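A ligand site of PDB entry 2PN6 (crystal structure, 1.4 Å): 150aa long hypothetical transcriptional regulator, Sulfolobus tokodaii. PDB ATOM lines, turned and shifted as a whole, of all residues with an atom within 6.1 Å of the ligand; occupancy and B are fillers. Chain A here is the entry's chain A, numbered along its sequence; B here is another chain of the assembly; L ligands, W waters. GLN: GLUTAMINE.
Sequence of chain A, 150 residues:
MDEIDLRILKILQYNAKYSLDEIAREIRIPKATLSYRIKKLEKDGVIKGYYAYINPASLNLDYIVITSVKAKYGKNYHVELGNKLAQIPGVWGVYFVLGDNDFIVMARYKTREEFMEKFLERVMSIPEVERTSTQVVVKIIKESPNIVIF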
ATOM      1  N   TYR A  73       5.345   2.427  -8.856  1.00  0.00           N
ATOM      2  CA  TYR A  73       5.595   3.858  -8.965  1.00  0.00           C
ATOM      3  C   TYR A  73       5.003   4.680  -7.837  1.00  0.00           C
ATOM      4  O   TYR A  73       3.951   4.362  -7.289  1.00  0.00           O
ATOM      5  CB  TYR A  73       5.086   4.379 -10.309  1.00  0.00           C
ATOM      6  CG  TYR A  73       5.983   4.054 -11.496  1.00  0.00           C
ATOM      7  CD1 TYR A  73       6.707   2.873 -11.549  1.00  0.00           C
ATOM      8  CD2 TYR A  73       6.064   4.928 -12.591  1.00  0.00           C
ATOM      9  CE1 TYR A  73       7.492   2.552 -12.667  1.00  0.00           C
ATOM     10  CE2 TYR A  73       6.834   4.619 -13.697  1.00  0.00           C
ATOM     11  CZ  TYR A  73       7.542   3.435 -13.734  1.00  0.00           C
ATOM     12  OH  TYR A  73       8.280   3.125 -14.857  1.00  0.00           O
ATOM     13  N   TYR A  77      10.301   7.174  -5.969  1.00  0.00           N
ATOM     14  CA  TYR A  77      10.498   5.747  -5.766  1.00  0.00           C
ATOM     15  C   TYR A  77      11.899   5.323  -6.187  1.00  0.00           C
ATOM     16  O   TYR A  77      12.464   4.383  -5.626  1.00  0.00           O
ATOM     17  CB  TYR A  77       9.455   4.939  -6.549  1.00  0.00           C
ATOM     18  CG  TYR A  77       9.813   4.684  -8.001  1.00  0.00           C
ATOM     19  CD1 TYR A  77      10.711   3.671  -8.353  1.00  0.00           C
ATOM     20  CD2 TYR A  77       9.286   5.466  -9.019  1.00  0.00           C
ATOM     21  CE1 TYR A  77      11.071   3.458  -9.675  1.00  0.00           C
ATOM     22  CE2 TYR A  77       9.646   5.266 -10.347  1.00  0.00           C
ATOM     23  CZ  TYR A  77      10.537   4.257 -10.668  1.00  0.00           C
ATOM     24  OH  TYR A  77      10.900   4.041 -11.977  1.00  0.00           O
ATOM     25  N   HIS A  78      12.478   6.015  -7.165  1.00  0.00           N
ATOM     26  CA  HIS A  78      13.812   5.667  -7.637  1.00  0.00           C
ATOM     27  C   HIS A  78      14.860   5.815  -6.536  1.00  0.00           C
ATOM     28  O   HIS A  78      15.793   5.020  -6.447  1.00  0.00           O
ATOM     29  CB  HIS A  78      14.186   6.506  -8.871  1.00  0.00           C
ATOM     30  CG  HIS A  78      14.199   7.986  -8.636  1.00  0.00           C
ATOM     31  ND1 HIS A  78      13.214   8.627  -7.915  1.00  0.00           N
ATOM     32  CD2 HIS A  78      15.025   8.948  -9.091  1.00  0.00           C
ATOM     33  CE1 HIS A  78      13.451   9.928  -7.926  1.00  0.00           C
ATOM     34  NE2 HIS A  78      14.542  10.149  -8.632  1.00  0.00           N
ATOM     35  N   PHE A  96      19.476   2.991 -12.360  1.00  0.00           N
ATOM     36  CA  PHE A  96      18.106   3.455 -12.626  1.00  0.00           C
ATOM     37  C   PHE A  96      18.084   3.614 -14.141  1.00  0.00           C
ATOM     38  O   PHE A  96      18.845   4.406 -14.713  1.00  0.00           O
ATOM     39  CB  PHE A  96      17.864   4.780 -11.903  1.00  0.00           C
ATOM     40  CG  PHE A  96      16.512   5.379 -12.158  1.00  0.00           C
ATOM     41  CD1 PHE A  96      15.357   4.610 -12.113  1.00  0.00           C
ATOM     42  CD2 PHE A  96      16.398   6.736 -12.459  1.00  0.00           C
ATOM     43  CE1 PHE A  96      14.103   5.187 -12.344  1.00  0.00           C
ATOM     44  CE2 PHE A  96      15.150   7.321 -12.689  1.00  0.00           C
ATOM     45  CZ  PHE A  96      14.001   6.547 -12.639  1.00  0.00           C
ATOM     46  N   VAL A  97      17.206   2.856 -14.805  1.00  0.00           N
ATOM     47  CA  VAL A  97      17.176   2.846 -16.266  1.00  0.00           C
ATOM     48  C   VAL A  97      15.878   3.176 -16.991  1.00  0.00           C
ATOM     49  O   VAL A  97      14.783   3.160 -16.419  1.00  0.00           O
ATOM     50  CB  VAL A  97      17.621   1.452 -16.785  1.00  0.00           C
ATOM     51  CG1 VAL A  97      19.066   1.175 -16.379  1.00  0.00           C
ATOM     52  CG2 VAL A  97      16.700   0.357 -16.227  1.00  0.00           C
ATOM     53  N   LEU A  98      16.040   3.490 -18.273  1.00  0.00           N
ATOM     54  CA  LEU A  98      14.910   3.777 -19.155  1.00  0.00           C
ATOM     55  C   LEU A  98      14.612   2.474 -19.888  1.00  0.00           C
ATOM     56  O   LEU A  98      15.534   1.755 -20.271  1.00  0.00           O
ATOM     57  CB  LEU A  98      15.280   4.871 -20.161  1.00  0.00           C
ATOM     58  CG  LEU A  98      15.643   6.230 -19.566  1.00  0.00           C
ATOM     59  CD1 LEU A  98      15.877   7.241 -20.687  1.00  0.00           C
ATOM     60  CD2 LEU A  98      14.509   6.701 -18.652  1.00  0.00           C
ATOM     61  N   GLY A  99      13.337   2.186 -20.076  1.00  0.00           N
ATOM     62  CA  GLY A  99      12.931   0.972 -20.756  1.00  0.00           C
ATOM     63  C   GLY A  99      11.811   0.262 -20.013  1.00  0.00           C
ATOM     64  O   GLY A  99      11.195   0.851 -19.112  1.00  0.00           O
ATOM     65  N   ASP A 100      11.569  -0.996 -20.364  1.00  0.00           N
ATOM     66  CA  ASP A 100      10.509  -1.794 -19.759  1.00  0.00           C
ATOM     67  C   ASP A 100      10.744  -2.181 -18.299  1.00  0.00           C
ATOM     68  O   ASP A 100       9.897  -2.814 -17.674  1.00  0.00           O
ATOM     69  CB  ASP A 100      10.256  -3.065 -20.575  1.00  0.00           C
ATOM     70  CG  ASP A 100       9.528  -2.795 -21.865  1.00  0.00           C
ATOM     71  OD1 ASP A 100       9.234  -1.616 -22.164  1.00  0.00           O
ATOM     72  OD2 ASP A 100       9.230  -3.764 -22.598  1.00  0.00           O
ATOM     73  N   ASN A 101      11.921  -1.846 -17.777  1.00  0.00           N
ATOM     74  CA  ASN A 101      12.232  -2.112 -16.391  1.00  0.00           C
ATOM     75  C   ASN A 101      12.771  -0.806 -15.826  1.00  0.00           C
ATOM     76  O   ASN A 101      13.118   0.096 -16.575  1.00  0.00           O
ATOM     77  CB  ASN A 101      13.247  -3.253 -16.267  1.00  0.00           C
ATOM     78  CG  ASN A 101      12.642  -4.593 -16.653  1.00  0.00           C
ATOM     79  OD1 ASN A 101      11.745  -5.104 -15.979  1.00  0.00           O
ATOM     80  ND2 ASN A 101      13.108  -5.164 -17.758  1.00  0.00           N
ATOM     81  N   ASP A 102      12.826  -0.710 -14.501  1.00  0.00           N
ATOM     82  CA  ASP A 102      13.265   0.531 -13.872  1.00  0.00           C
ATOM     83  C   ASP A 102      14.646   0.479 -13.248  1.00  0.00           C
ATOM     84  O   ASP A 102      15.310   1.513 -13.114  1.00  0.00           O
ATOM     85  CB  ASP A 102      12.204   0.957 -12.868  1.00  0.00           C
ATOM     86  CG  ASP A 102      10.817   0.939 -13.459  1.00  0.00           C
ATOM     87  OD1 ASP A 102      10.611   1.647 -14.483  1.00  0.00           O
ATOM     88  OD2 ASP A 102       9.941   0.208 -12.946  1.00  0.00           O
ATOM     89  N   THR B  67       7.881   8.310 -24.807  1.00  0.00           N
ATOM     90  CA  THR B  67       7.540   7.476 -23.664  1.00  0.00           C
ATOM     91  C   THR B  67       6.186   6.808 -23.760  1.00  0.00           C
ATOM     92  O   THR B  67       5.179   7.465 -24.018  1.00  0.00           O
ATOM     93  CB  THR B  67       7.608   8.318 -22.356  1.00  0.00           C
ATOM     94  OG1 THR B  67       8.934   8.818 -22.180  1.00  0.00           O
ATOM     95  CG2 THR B  67       7.214   7.494 -21.138  1.00  0.00           C
ATOM     96  N   SER B  68       6.169   5.500 -23.547  1.00  0.00           N
ATOM     97  CA  SER B  68       4.939   4.726 -23.563  1.00  0.00           C
ATOM     98  C   SER B  68       4.468   4.643 -22.124  1.00  0.00           C
ATOM     99  O   SER B  68       5.271   4.432 -21.206  1.00  0.00           O
ATOM    100  CB  SER B  68       5.198   3.319 -24.105  1.00  0.00           C
ATOM    101  OG  SER B  68       5.648   3.376 -25.451  1.00  0.00           O
ATOM    102  N   PHE B 115      15.734  16.044 -17.923  1.00  0.00           N
ATOM    103  CA  PHE B 115      14.725  15.046 -18.241  1.00  0.00           C
ATOM    104  C   PHE B 115      14.292  14.324 -16.972  1.00  0.00           C
ATOM    105  O   PHE B 115      13.101  14.094 -16.744  1.00  0.00           O
ATOM    106  CB  PHE B 115      15.324  14.091 -19.283  1.00  0.00           C
ATOM    107  CG  PHE B 115      14.619  12.777 -19.387  1.00  0.00           C
ATOM    108  CD1 PHE B 115      13.337  12.679 -19.906  1.00  0.00           C
ATOM    109  CD2 PHE B 115      15.277  11.614 -19.007  1.00  0.00           C
ATOM    110  CE1 PHE B 115      12.708  11.434 -20.042  1.00  0.00           C
ATOM    111  CE2 PHE B 115      14.673  10.364 -19.140  1.00  0.00           C
ATOM    112  CZ  PHE B 115      13.385  10.282 -19.655  1.00  0.00           C
ATOM    113  N   PHE B 119      10.605  15.590 -16.038  1.00  0.00           N
ATOM    114  CA  PHE B 119       9.720  14.558 -16.563  1.00  0.00           C
ATOM    115  C   PHE B 119       9.607  13.309 -15.710  1.00  0.00           C
ATOM    116  O   PHE B 119       8.535  13.030 -15.175  1.00  0.00           O
ATOM    117  CB  PHE B 119      10.177  14.192 -17.983  1.00  0.00           C
ATOM    118  CG  PHE B 119       9.252  13.234 -18.685  1.00  0.00           C
ATOM    119  CD1 PHE B 119       8.072  13.683 -19.259  1.00  0.00           C
ATOM    120  CD2 PHE B 119       9.576  11.887 -18.787  1.00  0.00           C
ATOM    121  CE1 PHE B 119       7.223  12.804 -19.926  1.00  0.00           C
ATOM    122  CE2 PHE B 119       8.733  10.992 -19.456  1.00  0.00           C
ATOM    123  CZ  PHE B 119       7.564  11.457 -20.030  1.00  0.00           C
ATOM    124  N   LEU B 120      10.689  12.551 -15.566  1.00  0.00           N
ATOM    125  CA  LEU B 120      10.621  11.309 -14.799  1.00  0.00           C
ATOM    126  C   LEU B 120      10.105  11.471 -13.386  1.00  0.00           C
ATOM    127  O   LEU B 120       9.222  10.725 -12.954  1.00  0.00           O
ATOM    128  CB  LEU B 120      11.991  10.631 -14.755  1.00  0.00           C
ATOM    129  CG  LEU B 120      12.604  10.147 -16.073  1.00  0.00           C
ATOM    130  CD1 LEU B 120      13.936   9.486 -15.759  1.00  0.00           C
ATOM    131  CD2 LEU B 120      11.680   9.151 -16.774  1.00  0.00           C
ATOM    132  N   GLU B 121      10.636  12.444 -12.662  1.00  0.00           N
ATOM    133  CA  GLU B 121      10.213  12.651 -11.287  1.00  0.00           C
ATOM    134  C   GLU B 121       8.772  13.151 -11.151  1.00  0.00           C
ATOM    135  O   GLU B 121       8.151  12.983 -10.107  1.00  0.00           O
ATOM    136  CB  GLU B 121      11.212  13.554 -10.561  1.00  0.00           C
ATOM    137  CG  GLU B 121      12.499  12.789 -10.234  1.00  0.00           C
ATOM    138  CD  GLU B 121      13.604  13.646  -9.649  1.00  0.00           C
ATOM    139  OE1 GLU B 121      13.343  14.813  -9.296  1.00  0.00           O
ATOM    140  OE2 GLU B 121      14.735  13.126  -9.528  1.00  0.00           O
ATOM    141  N   VAL B 123       6.277  12.275 -13.552  1.00  0.00           N
ATOM    142  CA  VAL B 123       5.460  11.141 -13.980  1.00  0.00           C
ATOM    143  C   VAL B 123       5.327  10.059 -12.924  1.00  0.00           C
ATOM    144  O   VAL B 123       4.246   9.491 -12.744  1.00  0.00           O
ATOM    145  CB  VAL B 123       6.026  10.505 -15.271  1.00  0.00           C
ATOM    146  CG1 VAL B 123       5.258   9.232 -15.613  1.00  0.00           C
ATOM    147  CG2 VAL B 123       5.928  11.499 -16.420  1.00  0.00           C
ATOM    148  N   MET B 124       6.413   9.773 -12.208  1.00  0.00           N
ATOM    149  CA  MET B 124       6.348   8.730 -11.200  1.00  0.00           C
ATOM    150  C   MET B 124       5.391   9.026 -10.059  1.00  0.00           C
ATOM    151  O   MET B 124       4.998   8.109  -9.341  1.00  0.00           O
ATOM    152  CB  MET B 124       7.752   8.416 -10.649  1.00  0.00           C
ATOM    153  CG  MET B 124       8.410   9.567  -9.895  1.00  0.00           C
ATOM    154  SD  MET B 124      10.022   9.109  -9.218  1.00  0.00           S
ATOM    155  CE  MET B 124      10.993   8.829 -10.715  1.00  0.00           C
ATOM    156  N   THR B 132       5.945   3.224 -16.980  1.00  0.00           N
ATOM    157  CA  THR B 132       6.254   3.779 -18.292  1.00  0.00           C
ATOM    158  C   THR B 132       7.529   3.154 -18.840  1.00  0.00           C
ATOM    159  O   THR B 132       8.303   2.538 -18.103  1.00  0.00           O
ATOM    160  CB  THR B 132       6.433   5.319 -18.263  1.00  0.00           C
ATOM    161  OG1 THR B 132       7.593   5.669 -17.482  1.00  0.00           O
ATOM    162  CG2 THR B 132       5.219   5.983 -17.661  1.00  0.00           C
ATOM    163  N   SER B 133       7.711   3.294 -20.144  1.00  0.00           N
ATOM    164  CA  SER B 133       8.889   2.795 -20.824  1.00  0.00           C
ATOM    165  C   SER B 133       9.299   3.895 -21.799  1.00  0.00           C
ATOM    166  O   SER B 133       8.570   4.226 -22.732  1.00  0.00           O
ATOM    167  CB  SER B 133       8.581   1.512 -21.582  1.00  0.00           C
ATOM    168  OG  SER B 133       9.739   1.066 -22.279  1.00  0.00           O
ATOM    169  N   THR B 134      10.477   4.463 -21.560  1.00  0.00           N
ATOM    170  CA  THR B 134      10.963   5.551 -22.382  1.00  0.00           C
ATOM    171  C   THR B 134      11.950   5.119 -23.449  1.00  0.00           C
ATOM    172  O   THR B 134      12.931   4.430 -23.170  1.00  0.00           O
ATOM    173  CB  THR B 134      11.630   6.629 -21.504  1.00  0.00           C
ATOM    174  OG1 THR B 134      10.651   7.172 -20.603  1.00  0.00           O
ATOM    175  CG2 THR B 134      12.198   7.745 -22.364  1.00  0.00           C
ATOM    176  N   GLN B 135      11.658   5.514 -24.681  1.00  0.00           N
ATOM    177  CA  GLN B 135      12.504   5.226 -25.825  1.00  0.00           C
ATOM    178  C   GLN B 135      13.281   6.492 -26.152  1.00  0.00           C
ATOM    179  O   GLN B 135      12.689   7.507 -26.516  1.00  0.00           O
ATOM    180  CB  GLN B 135      11.656   4.800 -27.030  1.00  0.00           C
ATOM    181  CG  GLN B 135      11.039   3.425 -26.912  1.00  0.00           C
ATOM    182  CD  GLN B 135      10.117   3.089 -28.069  1.00  0.00           C
ATOM    183  OE1 GLN B 135       8.905   3.289 -28.002  1.00  0.00           O
ATOM    184  NE2 GLN B 135      10.697   2.608 -29.157  1.00  0.00           N
HETATM  185  N   GLN L   1      11.804   2.770 -16.768  1.00  0.00           N
HETATM  186  CA  GLN L   1      10.818   3.889 -16.857  1.00  0.00           C
HETATM  187  C   GLN L   1      10.902   4.560 -18.222  1.00  0.00           C
HETATM  188  O   GLN L   1      10.060   5.445 -18.508  1.00  0.00           O
HETATM  189  CB  GLN L   1      11.068   4.915 -15.731  1.00  0.00           C
HETATM  190  CG  GLN L   1       9.977   5.992 -15.671  1.00  0.00           C
HETATM  191  CD  GLN L   1       9.977   6.848 -14.394  1.00  0.00           C
HETATM  192  OE1 GLN L   1       9.382   7.925 -14.377  1.00  0.00           O
HETATM  193  NE2 GLN L   1      10.614   6.368 -13.339  1.00  0.00           N
HETATM  194  OXT GLN L   1      11.794   4.186 -19.003  1.00  0.00           O
HETATM  195  O   HOH W   1       8.151   8.368 -17.089  1.00  0.00           O
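The side-chain hydroxyl (OG1) of Thr 132 of chain B sits at hydrogen-bond distance from an oxygen (O) of the ligand (2.7 Å).
OH of Tyr 77 sits at hydrogen-bond distance from NE2 of the ligand, 2.7 Å away.
An oxygen (OXT) of the ligand sits at hydrogen-bond distance from the backbone NH (N) of Gly 99 (2.7 Å).
A nitrogen (N) of the ligand lies within hydrogen-bond range of the backbone carbonyl oxygen (O) of Gly 99 (3.1 Å).
An oxygen (OXT) of the ligand sits at hydrogen-bond distance from the backbone NH of Thr 134 of chain B.
OG1 of Thr 134 of chain B lies within hydrogen-bond range of O of the ligand (2.8 Å).
N of the ligand lies within salt-bridge range of OD1 of Asp 102.
A nitrogen (N) of the ligand sits at hydrogen-bond distance from the backbone carbonyl oxygen (O) of Asn 101 (3.0 Å).
The backbone carbonyl oxygen of Val 97 is in hydrogen-bond range of a nitrogen (N) of the ligand (3.0 Å).
Water W1 bridges the side-chain hydroxyl (OG1) of Thr 132 of chain B (2.8 Å) and an oxygen (OE1) of the ligand (3.0 Å).
OE1 of the ligand sits close to O of Leu 120 of chain B (3.1 Å).
Merely in contact with the ligand: Leu 98 (3.1 Å), Tyr 73 (3.3 Å), Phe 96 (3.5 Å), Ser 133 of chain B (3.6 Å) and Met 124 of chain B (3.6 Å).
13 residues have an atom within 4 Å of the ligand: Tyr 73, Tyr 77, Phe 96, Val 97, Leu 98, Gly 99, Asn 101, Asp 102, Leu 120 of chain B, Met 124 of chain B, Thr 132 of chain B, Ser 133 of chain B and Thr 134 of chain B.
The side-chain carboxylate (OD1) of Asp 102 sits close to the side-chain hydroxyl (OH) of Tyr 77, 3.5 Å away.
SD of Met 124 of chain B sits close to N of Tyr 77 (3.8 Å).
The backbone carbonyl oxygen (O) of Gly 99 sits close to the side-chain hydroxyl (OG) of Ser 133 of chain B (3.5 Å).
The backbone carbonyl oxygen (O) of Asp 102 lies within hydrogen-bond range of the backbone NH (N) of Val 97, 2.9 Å away.
The side-chain carboxylate (OD1) of Asp 102 lies within hydrogen-bond range of the side-chain hydroxyl (OH) of Tyr 73, 2.8 Å away.
The backbone NH (N) of Leu 120 of chain B sits at hydrogen-bond distance from the backbone carbonyl oxygen (O) of Phe 115 of chain B, at 3.1 Å.
The backbone NH of Ser 68 of chain B lies within hydrogen-bond range of the backbone carbonyl oxygen of Ser 133 of chain B, 2.8 Å away.
The side-chain sulfur (SD) of Met 124 of chain B sits at hydrogen-bond distance from a ring nitrogen (ND1) of His 78 (3.5 Å).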
